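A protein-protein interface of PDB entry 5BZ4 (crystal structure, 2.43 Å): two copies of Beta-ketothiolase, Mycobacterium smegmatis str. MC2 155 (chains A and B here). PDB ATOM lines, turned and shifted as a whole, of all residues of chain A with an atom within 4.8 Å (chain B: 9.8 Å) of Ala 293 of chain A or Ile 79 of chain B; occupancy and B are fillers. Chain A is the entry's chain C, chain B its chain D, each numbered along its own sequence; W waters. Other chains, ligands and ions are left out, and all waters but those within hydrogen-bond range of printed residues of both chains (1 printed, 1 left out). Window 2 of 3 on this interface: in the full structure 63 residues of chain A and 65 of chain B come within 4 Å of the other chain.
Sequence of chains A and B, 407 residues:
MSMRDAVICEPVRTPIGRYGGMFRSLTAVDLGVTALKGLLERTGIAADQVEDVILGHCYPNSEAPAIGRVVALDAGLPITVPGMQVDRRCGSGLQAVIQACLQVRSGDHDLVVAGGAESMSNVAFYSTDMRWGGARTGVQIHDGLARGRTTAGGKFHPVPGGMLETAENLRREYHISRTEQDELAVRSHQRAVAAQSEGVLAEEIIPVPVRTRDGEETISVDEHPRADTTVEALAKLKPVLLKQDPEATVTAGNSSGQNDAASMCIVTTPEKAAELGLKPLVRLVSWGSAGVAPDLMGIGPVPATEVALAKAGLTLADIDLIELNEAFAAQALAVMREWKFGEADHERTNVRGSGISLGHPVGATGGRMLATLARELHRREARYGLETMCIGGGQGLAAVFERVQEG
Water W1 lies within hydrogen-bond range of a ring nitrogen (NE2) of His 157 of chain A (2.5 Å) and the backbone carbonyl oxygen (O) of Leu 73 of chain B (3.3 Å).
Among the printed residues, merely in contact across the chains: His 157 of chain A with Ile 79 of chain B, Gly 291 of chain A with Arg 69 of chain B, Ala 293 of chain A with Ile 79 of chain B, Pro 294 of chain A with Arg 69 of chain B, Pro 294 of chain A with Leu 73 of chain B and Pro 294 of chain A with Ile 79 of chain B.
Hydrophobic or aromatic side chains of chain B that line the printed part of chain A: Leu 73 and Ile 79. Hydrophobic or aromatic side chains of chain A within 4 Å of the printed part of chain B: His 157, Ala 293 and Pro 294. Along chain A the printed residues that touch a printed residue of chain B span positions 157 to 394. Among the printed residues, no Asp or Glu carboxylate lies within 4 Å of a Lys or Arg side-chain nitrogen of the other chain.
The backbone carbonyl oxygen of Gly 394 of chain A lies within hydrogen-bond range of the backbone NH of Val 292 of chain A, at 3.1 Å. O of Ile 79 of chain B is in hydrogen-bond range of NH1 of Arg 69 of chain B (2.8 Å). NH1 of Arg 69 of chain B sits at hydrogen-bond distance from O of Val 81 of chain B (2.8 Å).
Of the printed residues of chain B, His 157 of chain A touches Ile 79. Printed residues of chain B within 4 Å of Gly 291 of chain A: Arg 69, Ile 79 and Thr 80. Of chain B, only Arg 69 and Ile 79 come within 4 Å of Val 292 of chain A. Of the printed residues of chain B, Ala 293 of chain A touches Ile 79 (3.7 Å). Pro 294 of chain A touches three residues of chain B. No residue of chain B comes within 4 Å of Asp 295 of chain A. Of the printed residues of chain A, Arg 69 of chain B touches Gly 291 (3.9 Å), Val 292 (2.8 Å), Pro 294 (3.9 Å) and Gly 394 (2.7 Å). Of the printed residues of chain A, Leu 73 of chain B touches Pro 294. Pro 78 of chain B touches none of the printed residues of chain A. Printed residues of chain A within 4 Å of Ile 79 of chain B: His 157, Gly 291, Val 292, Ala 293 and Pro 294. Printed residues of chain A within 4 Å of Thr 80 of chain B: Gly 291. Gly 83 of chain B touches none of the printed residues of chain A. The nearest residue of chain B that does not touch Ala 293 of chain A is Arg 69 of chain B (4.8 Å). The nearest residue of chain A that does not touch Ile 79 of chain B is Gly 394 of chain A (4.5 Å).
No position is printed for both chains. Of the 11 pairs that touch across the chains among the printed residues, none has its exchanged pair printed and touching as well.
O of Gly 291 of chain A sits close to O of Ile 79 of chain B. The backbone NH (N) of Val 292 of chain A sits at hydrogen-bond distance from the backbone carbonyl oxygen (O) of Ile 79 of chain B (3.3 Å). The guanidinium group (NH2) of Arg 69 of chain B is in hydrogen-bond range of the backbone carbonyl oxygen (O) of Gly 394 of chain A, 2.7 Å away. The backbone carbonyl oxygen (O) of Val 292 of chain A sits at hydrogen-bond distance from the guanidinium group (NH2) of Arg 69 of chain B (2.8 Å). The backbone carbonyl oxygen (O) of Thr 80 of chain B lies within hydrogen-bond range of the backbone NH (N) of Gly 291 of chain A (3.3 Å).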
ATOM      1  N   HIS A 157     -21.222  30.177  10.692  1.00  0.00           N
ATOM      2  CA  HIS A 157     -21.556  28.757  10.803  1.00  0.00           C
ATOM      3  C   HIS A 157     -20.341  27.908  10.483  1.00  0.00           C
ATOM      4  O   HIS A 157     -20.377  27.079   9.570  1.00  0.00           O
ATOM      5  CB  HIS A 157     -22.718  28.407   9.873  1.00  0.00           C
ATOM      6  CG  HIS A 157     -23.955  29.197  10.140  1.00  0.00           C
ATOM      7  ND1 HIS A 157     -24.954  28.762  11.001  1.00  0.00           N
ATOM      8  CD2 HIS A 157     -24.361  30.407   9.692  1.00  0.00           C
ATOM      9  CE1 HIS A 157     -25.910  29.660  11.047  1.00  0.00           C
ATOM     10  NE2 HIS A 157     -25.578  30.677  10.266  1.00  0.00           N
ATOM     11  N   GLY A 291     -32.740  24.655   2.557  1.00  0.00           N
ATOM     12  CA  GLY A 291     -31.595  25.083   3.342  1.00  0.00           C
ATOM     13  C   GLY A 291     -31.587  24.442   4.721  1.00  0.00           C
ATOM     14  O   GLY A 291     -32.563  24.577   5.462  1.00  0.00           O
ATOM     15  N   VAL A 292     -30.501  23.756   5.072  1.00  0.00           N
ATOM     16  CA  VAL A 292     -30.380  23.153   6.391  1.00  0.00           C
ATOM     17  C   VAL A 292     -29.164  23.746   7.090  1.00  0.00           C
ATOM     18  O   VAL A 292     -28.543  24.670   6.572  1.00  0.00           O
ATOM     19  CB  VAL A 292     -30.251  21.619   6.310  1.00  0.00           C
ATOM     20  CG1 VAL A 292     -31.476  21.013   5.618  1.00  0.00           C
ATOM     21  CG2 VAL A 292     -28.957  21.213   5.610  1.00  0.00           C
ATOM     22  N   ALA A 293     -28.810  23.231   8.261  1.00  0.00           N
ATOM     23  CA  ALA A 293     -27.673  23.794   8.995  1.00  0.00           C
ATOM     24  C   ALA A 293     -26.351  23.414   8.350  1.00  0.00           C
ATOM     25  O   ALA A 293     -26.153  22.269   7.957  1.00  0.00           O
ATOM     26  CB  ALA A 293     -27.698  23.350  10.437  1.00  0.00           C
ATOM     27  N   PRO A 294     -25.437  24.385   8.231  1.00  0.00           N
ATOM     28  CA  PRO A 294     -24.141  24.088   7.620  1.00  0.00           C
ATOM     29  C   PRO A 294     -23.356  22.993   8.332  1.00  0.00           C
ATOM     30  O   PRO A 294     -22.560  22.333   7.654  1.00  0.00           O
ATOM     31  CB  PRO A 294     -23.421  25.431   7.692  1.00  0.00           C
ATOM     32  CG  PRO A 294     -24.538  26.423   7.509  1.00  0.00           C
ATOM     33  CD  PRO A 294     -25.677  25.838   8.313  1.00  0.00           C
ATOM     34  N   ASP A 295     -23.577  22.785   9.634  1.00  0.00           N
ATOM     35  CA  ASP A 295     -22.923  21.679  10.349  1.00  0.00           C
ATOM     36  C   ASP A 295     -23.654  20.348  10.165  1.00  0.00           C
ATOM     37  O   ASP A 295     -23.165  19.312  10.602  1.00  0.00           O
ATOM     38  CB  ASP A 295     -22.763  21.997  11.854  1.00  0.00           C
ATOM     39  CG  ASP A 295     -24.103  22.149  12.605  1.00  0.00           C
ATOM     40  OD1 ASP A 295     -25.189  21.760  12.108  1.00  0.00           O
ATOM     41  OD2 ASP A 295     -24.064  22.631  13.757  1.00  0.00           O
ATOM     42  N   LEU A 296     -24.826  20.376   9.535  1.00  0.00           N
ATOM     43  CA  LEU A 296     -25.562  19.140   9.268  1.00  0.00           C
ATOM     44  C   LEU A 296     -26.068  19.025   7.849  1.00  0.00           C
ATOM     45  O   LEU A 296     -27.141  18.483   7.630  1.00  0.00           O
ATOM     46  CB  LEU A 296     -26.758  18.996  10.210  1.00  0.00           C
ATOM     47  CG  LEU A 296     -26.462  18.672  11.664  1.00  0.00           C
ATOM     48  CD1 LEU A 296     -27.758  18.766  12.452  1.00  0.00           C
ATOM     49  CD2 LEU A 296     -25.818  17.290  11.759  1.00  0.00           C
ATOM     50  N   MET A 297     -25.295  19.543   6.903  1.00  0.00           N
ATOM     51  CA  MET A 297     -25.599  19.487   5.477  1.00  0.00           C
ATOM     52  C   MET A 297     -26.190  18.191   4.932  1.00  0.00           C
ATOM     53  O   MET A 297     -26.817  18.203   3.874  1.00  0.00           O
ATOM     54  CB  MET A 297     -24.325  19.717   4.705  1.00  0.00           C
ATOM     55  CG  MET A 297     -23.679  18.358   4.499  1.00  0.00           C
ATOM     56  SD  MET A 297     -22.729  18.285   3.062  1.00  0.00           S
ATOM     57  CE  MET A 297     -21.952  19.824   3.647  1.00  0.00           C
ATOM     58  N   GLY A 394     -24.737  23.424   3.305  1.00  0.00           N
ATOM     59  CA  GLY A 394     -25.991  23.126   3.967  1.00  0.00           C
ATOM     60  C   GLY A 394     -27.178  23.398   3.081  1.00  0.00           C
ATOM     61  O   GLY A 394     -27.954  24.310   3.328  1.00  0.00           O
ATOM     62  N   ALA B  47     -37.172  37.578   6.527  1.00  0.00           N
ATOM     63  CA  ALA B  47     -36.082  36.880   5.860  1.00  0.00           C
ATOM     64  C   ALA B  47     -36.487  35.494   5.338  1.00  0.00           C
ATOM     65  O   ALA B  47     -35.965  35.049   4.318  1.00  0.00           O
ATOM     66  CB  ALA B  47     -34.897  36.774   6.802  1.00  0.00           C
ATOM     67  N   ASP B  48     -37.413  34.817   6.011  1.00  0.00           N
ATOM     68  CA  ASP B  48     -37.864  33.519   5.515  1.00  0.00           C
ATOM     69  C   ASP B  48     -38.945  33.656   4.438  1.00  0.00           C
ATOM     70  O   ASP B  48     -39.608  32.690   4.082  1.00  0.00           O
ATOM     71  CB  ASP B  48     -38.350  32.621   6.668  1.00  0.00           C
ATOM     72  CG  ASP B  48     -39.673  33.075   7.270  1.00  0.00           C
ATOM     73  OD1 ASP B  48     -39.875  34.295   7.467  1.00  0.00           O
ATOM     74  OD2 ASP B  48     -40.517  32.198   7.580  1.00  0.00           O
ATOM     75  N   VAL B  50     -37.722  34.700   1.655  1.00  0.00           N
ATOM     76  CA  VAL B  50     -36.760  34.530   0.582  1.00  0.00           C
ATOM     77  C   VAL B  50     -36.508  33.055   0.329  1.00  0.00           C
ATOM     78  O   VAL B  50     -36.080  32.313   1.216  1.00  0.00           O
ATOM     79  CB  VAL B  50     -35.444  35.247   0.901  1.00  0.00           C
ATOM     80  CG1 VAL B  50     -34.464  35.053  -0.216  1.00  0.00           C
ATOM     81  CG2 VAL B  50     -35.699  36.745   1.103  1.00  0.00           C
ATOM     82  N   GLU B  51     -36.780  32.635  -0.900  1.00  0.00           N
ATOM     83  CA  GLU B  51     -36.732  31.232  -1.234  1.00  0.00           C
ATOM     84  C   GLU B  51     -35.436  30.842  -1.958  1.00  0.00           C
ATOM     85  O   GLU B  51     -35.115  29.666  -2.055  1.00  0.00           O
ATOM     86  CB  GLU B  51     -37.967  30.876  -2.063  1.00  0.00           C
ATOM     87  CG  GLU B  51     -39.264  30.996  -1.290  1.00  0.00           C
ATOM     88  CD  GLU B  51     -40.447  30.505  -2.085  1.00  0.00           C
ATOM     89  OE1 GLU B  51     -40.566  29.276  -2.250  1.00  0.00           O
ATOM     90  OE2 GLU B  51     -41.262  31.330  -2.535  1.00  0.00           O
ATOM     91  N   ARG B  69     -25.621  31.682  -1.269  1.00  0.00           N
ATOM     92  CA  ARG B  69     -25.845  31.034   0.022  1.00  0.00           C
ATOM     93  C   ARG B  69     -24.926  31.589   1.116  1.00  0.00           C
ATOM     94  O   ARG B  69     -25.316  31.690   2.274  1.00  0.00           O
ATOM     95  CB  ARG B  69     -25.650  29.522  -0.130  1.00  0.00           C
ATOM     96  CG  ARG B  69     -25.506  28.756   1.169  1.00  0.00           C
ATOM     97  CD  ARG B  69     -26.833  28.507   1.841  1.00  0.00           C
ATOM     98  NE  ARG B  69     -26.667  27.628   2.988  1.00  0.00           N
ATOM     99  CZ  ARG B  69     -27.623  27.318   3.856  1.00  0.00           C
ATOM    100  NH1 ARG B  69     -28.827  27.841   3.732  1.00  0.00           N
ATOM    101  NH2 ARG B  69     -27.365  26.501   4.863  1.00  0.00           N
ATOM    102  N   ALA B  72     -26.246  35.054   1.820  1.00  0.00           N
ATOM    103  CA  ALA B  72     -27.436  34.802   2.615  1.00  0.00           C
ATOM    104  C   ALA B  72     -27.111  34.521   4.080  1.00  0.00           C
ATOM    105  O   ALA B  72     -27.704  35.127   4.963  1.00  0.00           O
ATOM    106  CB  ALA B  72     -28.210  33.640   2.030  1.00  0.00           C
ATOM    107  N   LEU B  73     -26.192  33.596   4.353  1.00  0.00           N
ATOM    108  CA  LEU B  73     -25.830  33.295   5.742  1.00  0.00           C
ATOM    109  C   LEU B  73     -25.070  34.437   6.415  1.00  0.00           C
ATOM    110  O   LEU B  73     -25.270  34.700   7.598  1.00  0.00           O
ATOM    111  CB  LEU B  73     -24.998  32.007   5.827  1.00  0.00           C
ATOM    112  CG  LEU B  73     -25.598  30.728   5.257  1.00  0.00           C
ATOM    113  CD1 LEU B  73     -24.615  29.597   5.362  1.00  0.00           C
ATOM    114  CD2 LEU B  73     -26.876  30.386   5.971  1.00  0.00           C
ATOM    115  N   ASP B  74     -24.194  35.110   5.675  1.00  0.00           N
ATOM    116  CA  ASP B  74     -23.434  36.225   6.237  1.00  0.00           C
ATOM    117  C   ASP B  74     -24.287  37.482   6.461  1.00  0.00           C
ATOM    118  O   ASP B  74     -23.891  38.381   7.211  1.00  0.00           O
ATOM    119  CB  ASP B  74     -22.237  36.547   5.340  1.00  0.00           C
ATOM    120  CG  ASP B  74     -21.050  35.648   5.611  1.00  0.00           C
ATOM    121  OD1 ASP B  74     -21.262  34.551   6.169  1.00  0.00           O
ATOM    122  OD2 ASP B  74     -19.915  36.042   5.270  1.00  0.00           O
ATOM    123  N   ALA B  75     -25.462  37.547   5.830  1.00  0.00           N
ATOM    124  CA  ALA B  75     -26.380  38.668   6.071  1.00  0.00           C
ATOM    125  C   ALA B  75     -27.339  38.315   7.196  1.00  0.00           C
ATOM    126  O   ALA B  75     -28.186  39.111   7.569  1.00  0.00           O
ATOM    127  CB  ALA B  75     -27.149  39.025   4.822  1.00  0.00           C
ATOM    128  N   GLY B  76     -27.199  37.108   7.732  1.00  0.00           N
ATOM    129  CA  GLY B  76     -27.999  36.680   8.861  1.00  0.00           C
ATOM    130  C   GLY B  76     -29.307  36.024   8.472  1.00  0.00           C
ATOM    131  O   GLY B  76     -30.162  35.802   9.329  1.00  0.00           O
ATOM    132  N   LEU B  77     -29.482  35.706   7.194  1.00  0.00           N
ATOM    133  CA  LEU B  77     -30.724  35.079   6.770  1.00  0.00           C
ATOM    134  C   LEU B  77     -30.723  33.671   7.346  1.00  0.00           C
ATOM    135  O   LEU B  77     -29.664  33.099   7.569  1.00  0.00           O
ATOM    136  CB  LEU B  77     -30.875  35.080   5.241  1.00  0.00           C
ATOM    137  CG  LEU B  77     -31.455  36.350   4.613  1.00  0.00           C
ATOM    138  CD1 LEU B  77     -30.575  37.527   4.934  1.00  0.00           C
ATOM    139  CD2 LEU B  77     -31.603  36.223   3.114  1.00  0.00           C
ATOM    140  N   PRO B  78     -31.904  33.126   7.641  1.00  0.00           N
ATOM    141  CA  PRO B  78     -31.958  31.832   8.324  1.00  0.00           C
ATOM    142  C   PRO B  78     -31.302  30.727   7.507  1.00  0.00           C
ATOM    143  O   PRO B  78     -31.161  30.894   6.298  1.00  0.00           O
ATOM    144  CB  PRO B  78     -33.460  31.580   8.486  1.00  0.00           C
ATOM    145  CG  PRO B  78     -34.146  32.574   7.618  1.00  0.00           C
ATOM    146  CD  PRO B  78     -33.232  33.736   7.497  1.00  0.00           C
ATOM    147  N   ILE B  79     -30.918  29.624   8.147  1.00  0.00           N
ATOM    148  CA  ILE B  79     -30.234  28.537   7.455  1.00  0.00           C
ATOM    149  C   ILE B  79     -31.129  27.832   6.443  1.00  0.00           C
ATOM    150  O   ILE B  79     -30.670  26.980   5.702  1.00  0.00           O
ATOM    151  CB  ILE B  79     -29.685  27.500   8.456  1.00  0.00           C
ATOM    152  CG1 ILE B  79     -30.751  27.105   9.458  1.00  0.00           C
ATOM    153  CG2 ILE B  79     -28.474  28.024   9.191  1.00  0.00           C
ATOM    154  CD1 ILE B  79     -30.316  26.006  10.377  1.00  0.00           C
ATOM    155  N   THR B  80     -32.406  28.179   6.428  1.00  0.00           N
ATOM    156  CA  THR B  80     -33.352  27.615   5.472  1.00  0.00           C
ATOM    157  C   THR B  80     -33.288  28.224   4.068  1.00  0.00           C
ATOM    158  O   THR B  80     -33.868  27.678   3.139  1.00  0.00           O
ATOM    159  CB  THR B  80     -34.797  27.780   5.965  1.00  0.00           C
ATOM    160  OG1 THR B  80     -34.952  29.062   6.593  1.00  0.00           O
ATOM    161  CG2 THR B  80     -35.137  26.688   6.945  1.00  0.00           C
ATOM    162  N   VAL B  81     -32.636  29.376   3.932  1.00  0.00           N
ATOM    163  CA  VAL B  81     -32.567  30.085   2.660  1.00  0.00           C
ATOM    164  C   VAL B  81     -31.430  29.539   1.793  1.00  0.00           C
ATOM    165  O   VAL B  81     -30.267  29.685   2.123  1.00  0.00           O
ATOM    166  CB  VAL B  81     -32.366  31.614   2.869  1.00  0.00           C
ATOM    167  CG1 VAL B  81     -32.329  32.352   1.531  1.00  0.00           C
ATOM    168  CG2 VAL B  81     -33.469  32.185   3.736  1.00  0.00           C
ATOM    169  N   PRO B  82     -31.768  28.908   0.670  1.00  0.00           N
ATOM    170  CA  PRO B  82     -30.758  28.443  -0.282  1.00  0.00           C
ATOM    171  C   PRO B  82     -30.115  29.580  -1.108  1.00  0.00           C
ATOM    172  O   PRO B  82     -30.603  30.709  -1.120  1.00  0.00           O
ATOM    173  CB  PRO B  82     -31.555  27.498  -1.188  1.00  0.00           C
ATOM    174  CG  PRO B  82     -32.887  27.331  -0.539  1.00  0.00           C
ATOM    175  CD  PRO B  82     -33.124  28.559   0.234  1.00  0.00           C
ATOM    176  N   GLY B  83     -29.014  29.278  -1.790  1.00  0.00           N
ATOM    177  CA  GLY B  83     -28.325  30.271  -2.595  1.00  0.00           C
ATOM    178  C   GLY B  83     -27.346  29.621  -3.559  1.00  0.00           C
ATOM    179  O   GLY B  83     -26.861  28.517  -3.315  1.00  0.00           O
HETATM  180  O   HOH W   1     -26.779  32.775   9.844  1.00  0.00           O
